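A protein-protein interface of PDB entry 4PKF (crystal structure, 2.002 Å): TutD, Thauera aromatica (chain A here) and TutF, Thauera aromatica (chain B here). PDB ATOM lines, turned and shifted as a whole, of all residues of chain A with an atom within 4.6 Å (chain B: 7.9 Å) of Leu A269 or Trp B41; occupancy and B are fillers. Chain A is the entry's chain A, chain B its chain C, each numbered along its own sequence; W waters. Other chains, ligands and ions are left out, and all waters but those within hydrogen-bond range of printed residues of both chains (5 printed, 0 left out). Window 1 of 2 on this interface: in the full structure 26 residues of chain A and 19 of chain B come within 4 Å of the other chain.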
ATOM      1  N   LEU A 107       2.899  18.314  -2.488  1.00  0.00           N
ATOM      2  CA  LEU A 107       1.870  17.290  -2.347  1.00  0.00           C
ATOM      3  C   LEU A 107       1.905  16.332  -3.535  1.00  0.00           C
ATOM      4  O   LEU A 107       2.399  16.675  -4.622  1.00  0.00           O
ATOM      5  CB  LEU A 107       0.492  17.924  -2.227  1.00  0.00           C
ATOM      6  CG  LEU A 107       0.396  19.024  -1.150  1.00  0.00           C
ATOM      7  CD1 LEU A 107      -1.045  19.523  -1.091  1.00  0.00           C
ATOM      8  CD2 LEU A 107       0.843  18.508   0.197  1.00  0.00           C
ATOM      9  N   VAL A 108       1.329  15.154  -3.342  1.00  0.00           N
ATOM     10  CA  VAL A 108       1.475  14.075  -4.300  1.00  0.00           C
ATOM     11  C   VAL A 108       0.102  13.520  -4.683  1.00  0.00           C
ATOM     12  O   VAL A 108      -0.760  13.341  -3.828  1.00  0.00           O
ATOM     13  CB  VAL A 108       2.371  12.920  -3.725  1.00  0.00           C
ATOM     14  CG1 VAL A 108       2.527  11.777  -4.758  1.00  0.00           C
ATOM     15  CG2 VAL A 108       3.741  13.436  -3.272  1.00  0.00           C
ATOM     16  N   LEU A 109      -0.091  13.262  -5.974  1.00  0.00           N
ATOM     17  CA  LEU A 109      -1.280  12.608  -6.484  1.00  0.00           C
ATOM     18  C   LEU A 109      -0.761  11.476  -7.377  1.00  0.00           C
ATOM     19  O   LEU A 109       0.165  11.699  -8.166  1.00  0.00           O
ATOM     20  CB  LEU A 109      -2.165  13.584  -7.286  1.00  0.00           C
ATOM     21  CG  LEU A 109      -3.388  12.921  -7.941  1.00  0.00           C
ATOM     22  CD1 LEU A 109      -4.205  12.208  -6.887  1.00  0.00           C
ATOM     23  CD2 LEU A 109      -4.257  13.944  -8.672  1.00  0.00           C
ATOM     24  N   GLN A 110      -1.305  10.266  -7.240  1.00  0.00           N
ATOM     25  CA  GLN A 110      -0.807   9.151  -8.057  1.00  0.00           C
ATOM     26  C   GLN A 110      -1.896   8.648  -8.982  1.00  0.00           C
ATOM     27  O   GLN A 110      -3.085   8.780  -8.693  1.00  0.00           O
ATOM     28  CB  GLN A 110      -0.295   7.987  -7.186  1.00  0.00           C
ATOM     29  CG  GLN A 110       0.825   8.366  -6.204  1.00  0.00           C
ATOM     30  CD  GLN A 110       1.575   7.139  -5.652  1.00  0.00           C
ATOM     31  OE1 GLN A 110       2.044   6.286  -6.416  1.00  0.00           O
ATOM     32  NE2 GLN A 110       1.691   7.061  -4.325  1.00  0.00           N
ATOM     33  N   GLU A 111      -1.499   7.994 -10.072  1.00  0.00           N
ATOM     34  CA  GLU A 111      -2.526   7.436 -10.932  1.00  0.00           C
ATOM     35  C   GLU A 111      -3.333   6.332 -10.232  1.00  0.00           C
ATOM     36  O   GLU A 111      -2.819   5.594  -9.358  1.00  0.00           O
ATOM     37  CB  GLU A 111      -1.929   6.916 -12.238  1.00  0.00           C
ATOM     38  CG  GLU A 111      -0.833   5.933 -12.099  1.00  0.00           C
ATOM     39  CD  GLU A 111      -0.414   5.382 -13.461  1.00  0.00           C
ATOM     40  OE1 GLU A 111       0.574   4.620 -13.514  1.00  0.00           O
ATOM     41  OE2 GLU A 111      -1.079   5.725 -14.468  1.00  0.00           O
ATOM     42  N   ARG A 265      -5.671  22.085  -0.489  1.00  0.00           N
ATOM     43  CA  ARG A 265      -4.624  22.209  -1.504  1.00  0.00           C
ATOM     44  C   ARG A 265      -4.365  20.854  -2.203  1.00  0.00           C
ATOM     45  O   ARG A 265      -3.992  20.788  -3.393  1.00  0.00           O
ATOM     46  CB  ARG A 265      -3.342  22.761  -0.864  1.00  0.00           C
ATOM     47  CG  ARG A 265      -2.244  23.106  -1.857  1.00  0.00           C
ATOM     48  CD  ARG A 265      -1.236  24.057  -1.244  1.00  0.00           C
ATOM     49  NE  ARG A 265      -0.474  23.420  -0.174  1.00  0.00           N
ATOM     50  CZ  ARG A 265       0.628  22.678  -0.352  1.00  0.00           C
ATOM     51  NH1 ARG A 265       1.150  22.474  -1.556  1.00  0.00           N
ATOM     52  NH2 ARG A 265       1.231  22.146   0.700  1.00  0.00           N
ATOM     53  N   GLN A 266      -4.549  19.777  -1.447  1.00  0.00           N
ATOM     54  CA  GLN A 266      -4.507  18.427  -2.010  1.00  0.00           C
ATOM     55  C   GLN A 266      -5.643  18.292  -3.016  1.00  0.00           C
ATOM     56  O   GLN A 266      -5.455  17.800  -4.144  1.00  0.00           O
ATOM     57  CB  GLN A 266      -4.621  17.367  -0.897  1.00  0.00           C
ATOM     58  CG  GLN A 266      -4.562  15.927  -1.448  1.00  0.00           C
ATOM     59  CD  GLN A 266      -3.130  15.509  -1.738  1.00  0.00           C
ATOM     60  OE1 GLN A 266      -2.229  15.785  -0.950  1.00  0.00           O
ATOM     61  NE2 GLN A 266      -2.911  14.863  -2.870  1.00  0.00           N
ATOM     62  N   GLY A 267      -6.821  18.752  -2.599  1.00  0.00           N
ATOM     63  CA  GLY A 267      -7.991  18.801  -3.446  1.00  0.00           C
ATOM     64  C   GLY A 267      -7.756  19.571  -4.736  1.00  0.00           C
ATOM     65  O   GLY A 267      -8.205  19.152  -5.811  1.00  0.00           O
ATOM     66  N   ARG A 268      -7.049  20.694  -4.633  1.00  0.00           N
ATOM     67  CA  ARG A 268      -6.807  21.558  -5.778  1.00  0.00           C
ATOM     68  C   ARG A 268      -5.878  20.891  -6.788  1.00  0.00           C
ATOM     69  O   ARG A 268      -6.035  21.085  -7.986  1.00  0.00           O
ATOM     70  CB  ARG A 268      -6.226  22.894  -5.313  1.00  0.00           C
ATOM     71  CG  ARG A 268      -5.939  23.850  -6.414  1.00  0.00           C
ATOM     72  CD  ARG A 268      -5.797  25.280  -5.832  1.00  0.00           C
ATOM     73  NE  ARG A 268      -4.475  25.487  -5.203  1.00  0.00           N
ATOM     74  CZ  ARG A 268      -4.281  25.886  -3.950  1.00  0.00           C
ATOM     75  NH1 ARG A 268      -3.042  26.065  -3.496  1.00  0.00           N
ATOM     76  NH2 ARG A 268      -5.312  26.117  -3.152  1.00  0.00           N
ATOM     77  N   LEU A 269      -4.952  20.063  -6.308  1.00  0.00           N
ATOM     78  CA  LEU A 269      -4.086  19.260  -7.169  1.00  0.00           C
ATOM     79  C   LEU A 269      -4.915  18.255  -7.981  1.00  0.00           C
ATOM     80  O   LEU A 269      -4.655  18.073  -9.167  1.00  0.00           O
ATOM     81  CB  LEU A 269      -2.992  18.543  -6.344  1.00  0.00           C
ATOM     82  CG  LEU A 269      -2.174  17.409  -6.993  1.00  0.00           C
ATOM     83  CD1 LEU A 269      -1.528  17.843  -8.302  1.00  0.00           C
ATOM     84  CD2 LEU A 269      -1.048  16.856  -6.052  1.00  0.00           C
ATOM     85  N   CYS A 270      -5.922  17.631  -7.371  1.00  0.00           N
ATOM     86  CA  CYS A 270      -6.835  16.770  -8.150  1.00  0.00           C
ATOM     87  C   CYS A 270      -7.538  17.554  -9.277  1.00  0.00           C
ATOM     88  O   CYS A 270      -7.640  17.082 -10.428  1.00  0.00           O
ATOM     89  CB  CYS A 270      -7.891  16.122  -7.240  1.00  0.00           C
ATOM     90  SG  CYS A 270      -7.235  14.877  -6.086  1.00  0.00           S
ATOM     91  N   LYS A 271      -8.048  18.731  -8.928  1.00  0.00           N
ATOM     92  CA  LYS A 271      -8.676  19.629  -9.897  1.00  0.00           C
ATOM     93  C   LYS A 271      -7.736  20.016 -11.028  1.00  0.00           C
ATOM     94  O   LYS A 271      -8.073  19.891 -12.204  1.00  0.00           O
ATOM     95  CB  LYS A 271      -9.195  20.872  -9.202  1.00  0.00           C
ATOM     96  CG  LYS A 271      -9.981  21.795 -10.151  1.00  0.00           C
ATOM     97  CD  LYS A 271     -10.498  23.035  -9.400  1.00  0.00           C
ATOM     98  CE  LYS A 271     -11.140  24.058 -10.335  1.00  0.00           C
ATOM     99  NZ  LYS A 271     -12.536  23.689 -10.764  1.00  0.00           N
ATOM    100  N   ILE A 272      -6.560  20.495 -10.674  1.00  0.00           N
ATOM    101  CA  ILE A 272      -5.556  20.822 -11.670  1.00  0.00           C
ATOM    102  C   ILE A 272      -5.183  19.647 -12.608  1.00  0.00           C
ATOM    103  O   ILE A 272      -5.065  19.841 -13.834  1.00  0.00           O
ATOM    104  CB  ILE A 272      -4.285  21.346 -10.996  1.00  0.00           C
ATOM    105  CG1 ILE A 272      -4.478  22.809 -10.566  1.00  0.00           C
ATOM    106  CG2 ILE A 272      -3.086  21.277 -11.962  1.00  0.00           C
ATOM    107  CD1 ILE A 272      -3.400  23.275  -9.559  1.00  0.00           C
ATOM    108  N   VAL A 273      -4.971  18.447 -12.059  1.00  0.00           N
ATOM    109  CA  VAL A 273      -4.661  17.280 -12.912  1.00  0.00           C
ATOM    110  C   VAL A 273      -5.845  16.933 -13.831  1.00  0.00           C
ATOM    111  O   VAL A 273      -5.648  16.659 -15.018  1.00  0.00           O
ATOM    112  CB  VAL A 273      -4.223  16.043 -12.071  1.00  0.00           C
ATOM    113  CG1 VAL A 273      -4.218  14.744 -12.919  1.00  0.00           C
ATOM    114  CG2 VAL A 273      -2.833  16.298 -11.514  1.00  0.00           C
ATOM    115  N   PHE A 277      -4.004  17.714 -17.159  1.00  0.00           N
ATOM    116  CA  PHE A 277      -3.087  16.617 -17.392  1.00  0.00           C
ATOM    117  C   PHE A 277      -3.796  15.333 -17.806  1.00  0.00           C
ATOM    118  O   PHE A 277      -3.313  14.587 -18.646  1.00  0.00           O
ATOM    119  CB  PHE A 277      -2.255  16.347 -16.132  1.00  0.00           C
ATOM    120  CG  PHE A 277      -1.280  17.437 -15.796  1.00  0.00           C
ATOM    121  CD1 PHE A 277      -1.685  18.546 -15.066  1.00  0.00           C
ATOM    122  CD2 PHE A 277       0.052  17.328 -16.162  1.00  0.00           C
ATOM    123  CE1 PHE A 277      -0.801  19.551 -14.748  1.00  0.00           C
ATOM    124  CE2 PHE A 277       0.961  18.318 -15.831  1.00  0.00           C
ATOM    125  CZ  PHE A 277       0.536  19.434 -15.127  1.00  0.00           C
ATOM    126  N   ASN B  11       5.092  23.647 -14.817  1.00  0.00           N
ATOM    127  CA  ASN B  11       3.743  24.203 -14.973  1.00  0.00           C
ATOM    128  C   ASN B  11       3.231  24.990 -13.763  1.00  0.00           C
ATOM    129  O   ASN B  11       3.229  24.504 -12.637  1.00  0.00           O
ATOM    130  CB  ASN B  11       2.765  23.092 -15.277  1.00  0.00           C
ATOM    131  CG  ASN B  11       3.151  22.311 -16.508  1.00  0.00           C
ATOM    132  OD1 ASN B  11       2.733  22.651 -17.621  1.00  0.00           O
ATOM    133  ND2 ASN B  11       3.949  21.249 -16.319  1.00  0.00           N
ATOM    134  N   ASP B  28       0.779  27.234  -7.467  1.00  0.00           N
ATOM    135  CA  ASP B  28       1.164  25.810  -7.435  1.00  0.00           C
ATOM    136  C   ASP B  28       2.002  25.477  -8.647  1.00  0.00           C
ATOM    137  O   ASP B  28       1.565  25.694  -9.775  1.00  0.00           O
ATOM    138  CB  ASP B  28      -0.045  24.874  -7.438  1.00  0.00           C
ATOM    139  CG  ASP B  28      -1.022  25.118  -6.294  1.00  0.00           C
ATOM    140  OD1 ASP B  28      -0.601  25.409  -5.150  1.00  0.00           O
ATOM    141  OD2 ASP B  28      -2.235  24.933  -6.546  1.00  0.00           O
ATOM    142  N   CYS B  29       3.200  24.959  -8.426  1.00  0.00           N
ATOM    143  CA  CYS B  29       4.003  24.399  -9.502  1.00  0.00           C
ATOM    144  C   CYS B  29       3.706  22.912  -9.574  1.00  0.00           C
ATOM    145  O   CYS B  29       3.949  22.177  -8.619  1.00  0.00           O
ATOM    146  CB  CYS B  29       5.494  24.638  -9.267  1.00  0.00           C
ATOM    147  SG  CYS B  29       6.552  23.843 -10.472  1.00  0.00           S
ATOM    148  N   VAL B  30       3.158  22.474 -10.697  1.00  0.00           N
ATOM    149  CA  VAL B  30       2.666  21.110 -10.820  1.00  0.00           C
ATOM    150  C   VAL B  30       3.445  20.448 -11.927  1.00  0.00           C
ATOM    151  O   VAL B  30       3.590  21.006 -13.018  1.00  0.00           O
ATOM    152  CB  VAL B  30       1.168  21.062 -11.120  1.00  0.00           C
ATOM    153  CG1 VAL B  30       0.688  19.597 -11.263  1.00  0.00           C
ATOM    154  CG2 VAL B  30       0.400  21.791 -10.037  1.00  0.00           C
ATOM    155  N   ARG B  31       3.992  19.278 -11.641  1.00  0.00           N
ATOM    156  CA  ARG B  31       4.678  18.549 -12.675  1.00  0.00           C
ATOM    157  C   ARG B  31       4.311  17.081 -12.617  1.00  0.00           C
ATOM    158  O   ARG B  31       3.976  16.523 -11.564  1.00  0.00           O
ATOM    159  CB  ARG B  31       6.202  18.769 -12.587  1.00  0.00           C
ATOM    160  CG  ARG B  31       6.847  18.442 -11.266  1.00  0.00           C
ATOM    161  CD  ARG B  31       8.055  19.389 -10.951  1.00  0.00           C
ATOM    162  NE  ARG B  31       8.961  18.773  -9.969  1.00  0.00           N
ATOM    163  CZ  ARG B  31       8.977  19.036  -8.656  1.00  0.00           C
ATOM    164  NH1 ARG B  31       8.157  19.932  -8.129  1.00  0.00           N
ATOM    165  NH2 ARG B  31       9.825  18.398  -7.858  1.00  0.00           N
ATOM    166  N   GLU B  32       4.320  16.478 -13.796  1.00  0.00           N
ATOM    167  CA  GLU B  32       4.041  15.073 -13.950  1.00  0.00           C
ATOM    168  C   GLU B  32       5.365  14.337 -13.956  1.00  0.00           C
ATOM    169  O   GLU B  32       6.332  14.809 -14.547  1.00  0.00           O
ATOM    170  CB  GLU B  32       3.260  14.828 -15.234  1.00  0.00           C
ATOM    171  CG  GLU B  32       2.851  13.381 -15.444  1.00  0.00           C
ATOM    172  CD  GLU B  32       1.997  13.229 -16.688  1.00  0.00           C
ATOM    173  OE1 GLU B  32       2.403  12.475 -17.580  1.00  0.00           O
ATOM    174  OE2 GLU B  32       0.945  13.892 -16.779  1.00  0.00           O
ATOM    175  N   LYS B  33       5.416  13.208 -13.252  1.00  0.00           N
ATOM    176  CA  LYS B  33       6.584  12.319 -13.284  1.00  0.00           C
ATOM    177  C   LYS B  33       6.135  10.893 -13.542  1.00  0.00           C
ATOM    178  O   LYS B  33       4.986  10.545 -13.291  1.00  0.00           O
ATOM    179  CB  LYS B  33       7.363  12.402 -11.974  1.00  0.00           C
ATOM    180  CG  LYS B  33       8.027  13.747 -11.741  1.00  0.00           C
ATOM    181  CD  LYS B  33       8.745  13.777 -10.400  1.00  0.00           C
ATOM    182  CE  LYS B  33      10.228  14.094 -10.539  1.00  0.00           C
ATOM    183  NZ  LYS B  33      11.027  12.987 -11.135  1.00  0.00           N
ATOM    184  N   GLU B  34       7.036  10.055 -14.037  1.00  0.00           N
ATOM    185  CA  GLU B  34       6.721   8.645 -14.186  1.00  0.00           C
ATOM    186  C   GLU B  34       7.995   7.827 -13.971  1.00  0.00           C
ATOM    187  O   GLU B  34       9.039   8.174 -14.511  1.00  0.00           O
ATOM    188  CB  GLU B  34       6.110   8.385 -15.561  1.00  0.00           C
ATOM    189  CG  GLU B  34       5.566   6.962 -15.768  1.00  0.00           C
ATOM    190  CD  GLU B  34       4.636   6.854 -16.990  1.00  0.00           C
ATOM    191  OE1 GLU B  34       4.594   7.798 -17.803  1.00  0.00           O
ATOM    192  OE2 GLU B  34       3.943   5.818 -17.133  1.00  0.00           O
ATOM    193  N   GLY B  38       4.990   3.837 -11.667  1.00  0.00           N
ATOM    194  CA  GLY B  38       3.883   4.459 -12.347  1.00  0.00           C
ATOM    195  C   GLY B  38       3.992   5.960 -12.418  1.00  0.00           C
ATOM    196  O   GLY B  38       5.044   6.554 -12.134  1.00  0.00           O
ATOM    197  N   LYS B  39       2.879   6.558 -12.814  1.00  0.00           N
ATOM    198  CA  LYS B  39       2.758   7.982 -13.071  1.00  0.00           C
ATOM    199  C   LYS B  39       2.287   8.720 -11.826  1.00  0.00           C
ATOM    200  O   LYS B  39       1.424   8.226 -11.085  1.00  0.00           O
ATOM    201  CB  LYS B  39       1.761   8.219 -14.208  1.00  0.00           C
ATOM    202  CG  LYS B  39       1.803   9.617 -14.800  1.00  0.00           C
ATOM    203  CD  LYS B  39       0.606   9.881 -15.746  1.00  0.00           C
ATOM    204  CE  LYS B  39       0.526   8.907 -16.901  1.00  0.00           C
ATOM    205  NZ  LYS B  39       1.257   9.410 -18.095  1.00  0.00           N
ATOM    206  N   TYR B  40       2.819   9.911 -11.602  1.00  0.00           N
ATOM    207  CA  TYR B  40       2.286  10.727 -10.521  1.00  0.00           C
ATOM    208  C   TYR B  40       2.482  12.230 -10.745  1.00  0.00           C
ATOM    209  O   TYR B  40       3.193  12.654 -11.663  1.00  0.00           O
ATOM    210  CB  TYR B  40       2.900  10.289  -9.184  1.00  0.00           C
ATOM    211  CG  TYR B  40       4.402  10.388  -9.076  1.00  0.00           C
ATOM    212  CD1 TYR B  40       5.214   9.311  -9.430  1.00  0.00           C
ATOM    213  CD2 TYR B  40       5.009  11.517  -8.563  1.00  0.00           C
ATOM    214  CE1 TYR B  40       6.600   9.373  -9.305  1.00  0.00           C
ATOM    215  CE2 TYR B  40       6.426  11.594  -8.422  1.00  0.00           C
ATOM    216  CZ  TYR B  40       7.201  10.516  -8.798  1.00  0.00           C
ATOM    217  OH  TYR B  40       8.583  10.554  -8.671  1.00  0.00           O
ATOM    218  N   TRP B  41       1.822  13.027  -9.915  1.00  0.00           N
ATOM    219  CA  TRP B  41       1.925  14.482 -10.011  1.00  0.00           C
ATOM    220  C   TRP B  41       2.342  15.066  -8.680  1.00  0.00           C
ATOM    221  O   TRP B  41       1.838  14.644  -7.645  1.00  0.00           O
ATOM    222  CB  TRP B  41       0.605  15.081 -10.460  1.00  0.00           C
ATOM    223  CG  TRP B  41       0.206  14.586 -11.818  1.00  0.00           C
ATOM    224  CD1 TRP B  41       0.468  15.184 -13.022  1.00  0.00           C
ATOM    225  CD2 TRP B  41      -0.498  13.376 -12.114  1.00  0.00           C
ATOM    226  NE1 TRP B  41      -0.026  14.425 -14.044  1.00  0.00           N
ATOM    227  CE2 TRP B  41      -0.629  13.306 -13.520  1.00  0.00           C
ATOM    228  CE3 TRP B  41      -1.021  12.340 -11.330  1.00  0.00           C
ATOM    229  CZ2 TRP B  41      -1.267  12.231 -14.165  1.00  0.00           C
ATOM    230  CZ3 TRP B  41      -1.661  11.274 -11.970  1.00  0.00           C
ATOM    231  CH2 TRP B  41      -1.771  11.230 -13.378  1.00  0.00           C
ATOM    232  N   LEU B  42       3.256  16.032  -8.737  1.00  0.00           N
ATOM    233  CA  LEU B  42       3.762  16.789  -7.601  1.00  0.00           C
ATOM    234  C   LEU B  42       3.288  18.258  -7.643  1.00  0.00           C
ATOM    235  O   LEU B  42       3.369  18.897  -8.706  1.00  0.00           O
ATOM    236  CB  LEU B  42       5.284  16.764  -7.597  1.00  0.00           C
ATOM    237  CG  LEU B  42       5.904  15.374  -7.537  1.00  0.00           C
ATOM    238  CD1 LEU B  42       7.406  15.492  -7.492  1.00  0.00           C
ATOM    239  CD2 LEU B  42       5.368  14.648  -6.328  1.00  0.00           C
ATOM    240  N   SER B  43       2.810  18.778  -6.506  1.00  0.00           N
ATOM    241  CA  SER B  43       2.362  20.180  -6.420  1.00  0.00           C
ATOM    242  C   SER B  43       3.091  20.904  -5.301  1.00  0.00           C
ATOM    243  O   SER B  43       2.836  20.632  -4.135  1.00  0.00           O
ATOM    244  CB  SER B  43       0.853  20.286  -6.171  1.00  0.00           C
ATOM    245  OG  SER B  43       0.468  21.660  -6.027  1.00  0.00           O
ATOM    246  N   LYS B  44       3.982  21.818  -5.677  1.00  0.00           N
ATOM    247  CA  LYS B  44       4.782  22.584  -4.737  1.00  0.00           C
ATOM    248  C   LYS B  44       4.430  24.062  -4.798  1.00  0.00           C
ATOM    249  O   LYS B  44       4.377  24.623  -5.881  1.00  0.00           O
ATOM    250  CB  LYS B  44       6.273  22.398  -5.048  1.00  0.00           C
ATOM    251  CG  LYS B  44       7.184  23.144  -4.050  1.00  0.00           C
ATOM    252  CD  LYS B  44       8.637  22.753  -4.229  1.00  0.00           C
ATOM    253  CE  LYS B  44       9.517  23.468  -3.225  1.00  0.00           C
ATOM    254  NZ  LYS B  44       9.090  24.877  -3.079  1.00  0.00           N
HETATM  255  O   HOH W   1       0.934  23.420  -4.026  1.00  0.00           O
HETATM  256  O   HOH W   2      -1.239  12.539 -18.077  1.00  0.00           O
HETATM  257  O   HOH W   3       2.521   6.047  -9.305  1.00  0.00           O
HETATM  258  O   HOH W   4      -2.285  21.922  -5.426  1.00  0.00           O
HETATM  259  O   HOH W   5      -3.434  26.664  -8.024  1.00  0.00           O
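The side-chain carboxylate of Glu A111 is in hydrogen-bond range of the backbone NH of Lys B39 (3.1 Å).
The backbone carbonyl oxygen of Leu A109 sits at hydrogen-bond distance from the backbone NH of Trp B41, 2.8 Å away.
O of Ser B43 is in hydrogen-bond range of N of Leu A107 (2.8 Å).
The guanidinium group (NE) of Arg A268 is in salt-bridge range of the side-chain carboxylate (OD2) of Asp B28, at 2.7 Å.
The backbone NH (N) of Leu B42 sits at hydrogen-bond distance from the backbone carbonyl oxygen (O) of Arg B31, 3.0 Å away.
O of Asn B11 sits at hydrogen-bond distance from N of Val B30, at 2.8 Å.
The backbone NH of Lys B33 lies within hydrogen-bond range of the backbone carbonyl oxygen of Tyr B40 (2.8 Å).
The side-chain carboxylate of Glu B32 is in salt-bridge range of the side-chain amino group of Lys B39, at 3.3 Å.
O of Val A108 is in hydrogen-bond range of NE2 of Gln A266, at 2.8 Å.
NZ of Lys B39 lies within salt-bridge range of OE1 of Glu B34 (3.7 Å).
O of Leu A107 touches O of Trp B41 (3.7 Å).
Leu A107 touches Leu B42 (O to CA, 3.3 Å).
CD2 of Leu B42 touches CG2 of Val A108, 3.7 Å away.
CB of Tyr B40 touches O of Leu A109 (3.2 Å).
Gln A110 touches Lys B39.
Trp B41 touches Gln A110.
Arg A265 touches Ser B43 (NH1 to O, 3.6 Å).
Asp B28 touches Ile A272 (OD2 to CD1, 3.6 Å).
CG1 of Val B30 touches CE1 of Phe A277, 3.8 Å away.
Phe A277 touches Trp B41.
Of chain B, only Trp B41 (3.97 Å) and Ser B43 (3.9 Å) come within 4 Å of Leu A269.
Of the printed residues of chain A, Trp B41 touches Leu A107, Val A108, Leu A109, Gln A110, Glu A111, Leu A269, Val A273 and Phe A277.
Of the printed residues of chain A, Glu B32 touches Phe A277.
Printed residues of chain B within 4 Å of Arg A268: Asp B28.
Printed residues of chain B within 4 Å of Gln A110: Lys B39 (3.9 Å) and Trp B41 (3.98 Å).
Glu B34 touches none of the printed residues of chain A.
Lys B44 touches none of the printed residues of chain A.
The nearest residue of chain B that does not touch Leu A269 is Val B30 (4.1 Å).
The nearest printed residue of chain A that does not touch Trp B41 is Gln A266 (6.7 Å).
Of the 15 printed residues of chain A, 11 touch a printed residue of chain B.
Hydrophobic or aromatic side chains of chain B within 4 Å of the printed part of chain A: Val B30, Tyr B40, Trp B41 and Leu B42.
Water W5 bridges OD2 of Asp B28 (2.6 Å) and NE of Arg A268 (3.2 Å).
Water W1 lies within hydrogen-bond range of the guanidinium group of Arg A265 (2.7 Å), the side-chain hydroxyl of Ser B43 (2.7 Å) and the side-chain carboxylate of Asp B28 (2.8 Å).
Water W4 lies within hydrogen-bond range of OG of Ser B43 (2.8 Å), O of Arg A265 (2.9 Å), OD2 of Asp B28 (3.2 Å) and N of Leu A269 (3.4 Å).
Water W2 bridges the side-chain carboxylate of Glu B32 (2.9 Å) and the backbone carbonyl oxygen of Phe A277 (3.0 Å).
Water W3 lies within hydrogen-bond range of the side-chain amide oxygen (OE1) of Gln A110 (2.9 Å) and the backbone carbonyl oxygen (O) of Lys B39 (3.0 Å).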
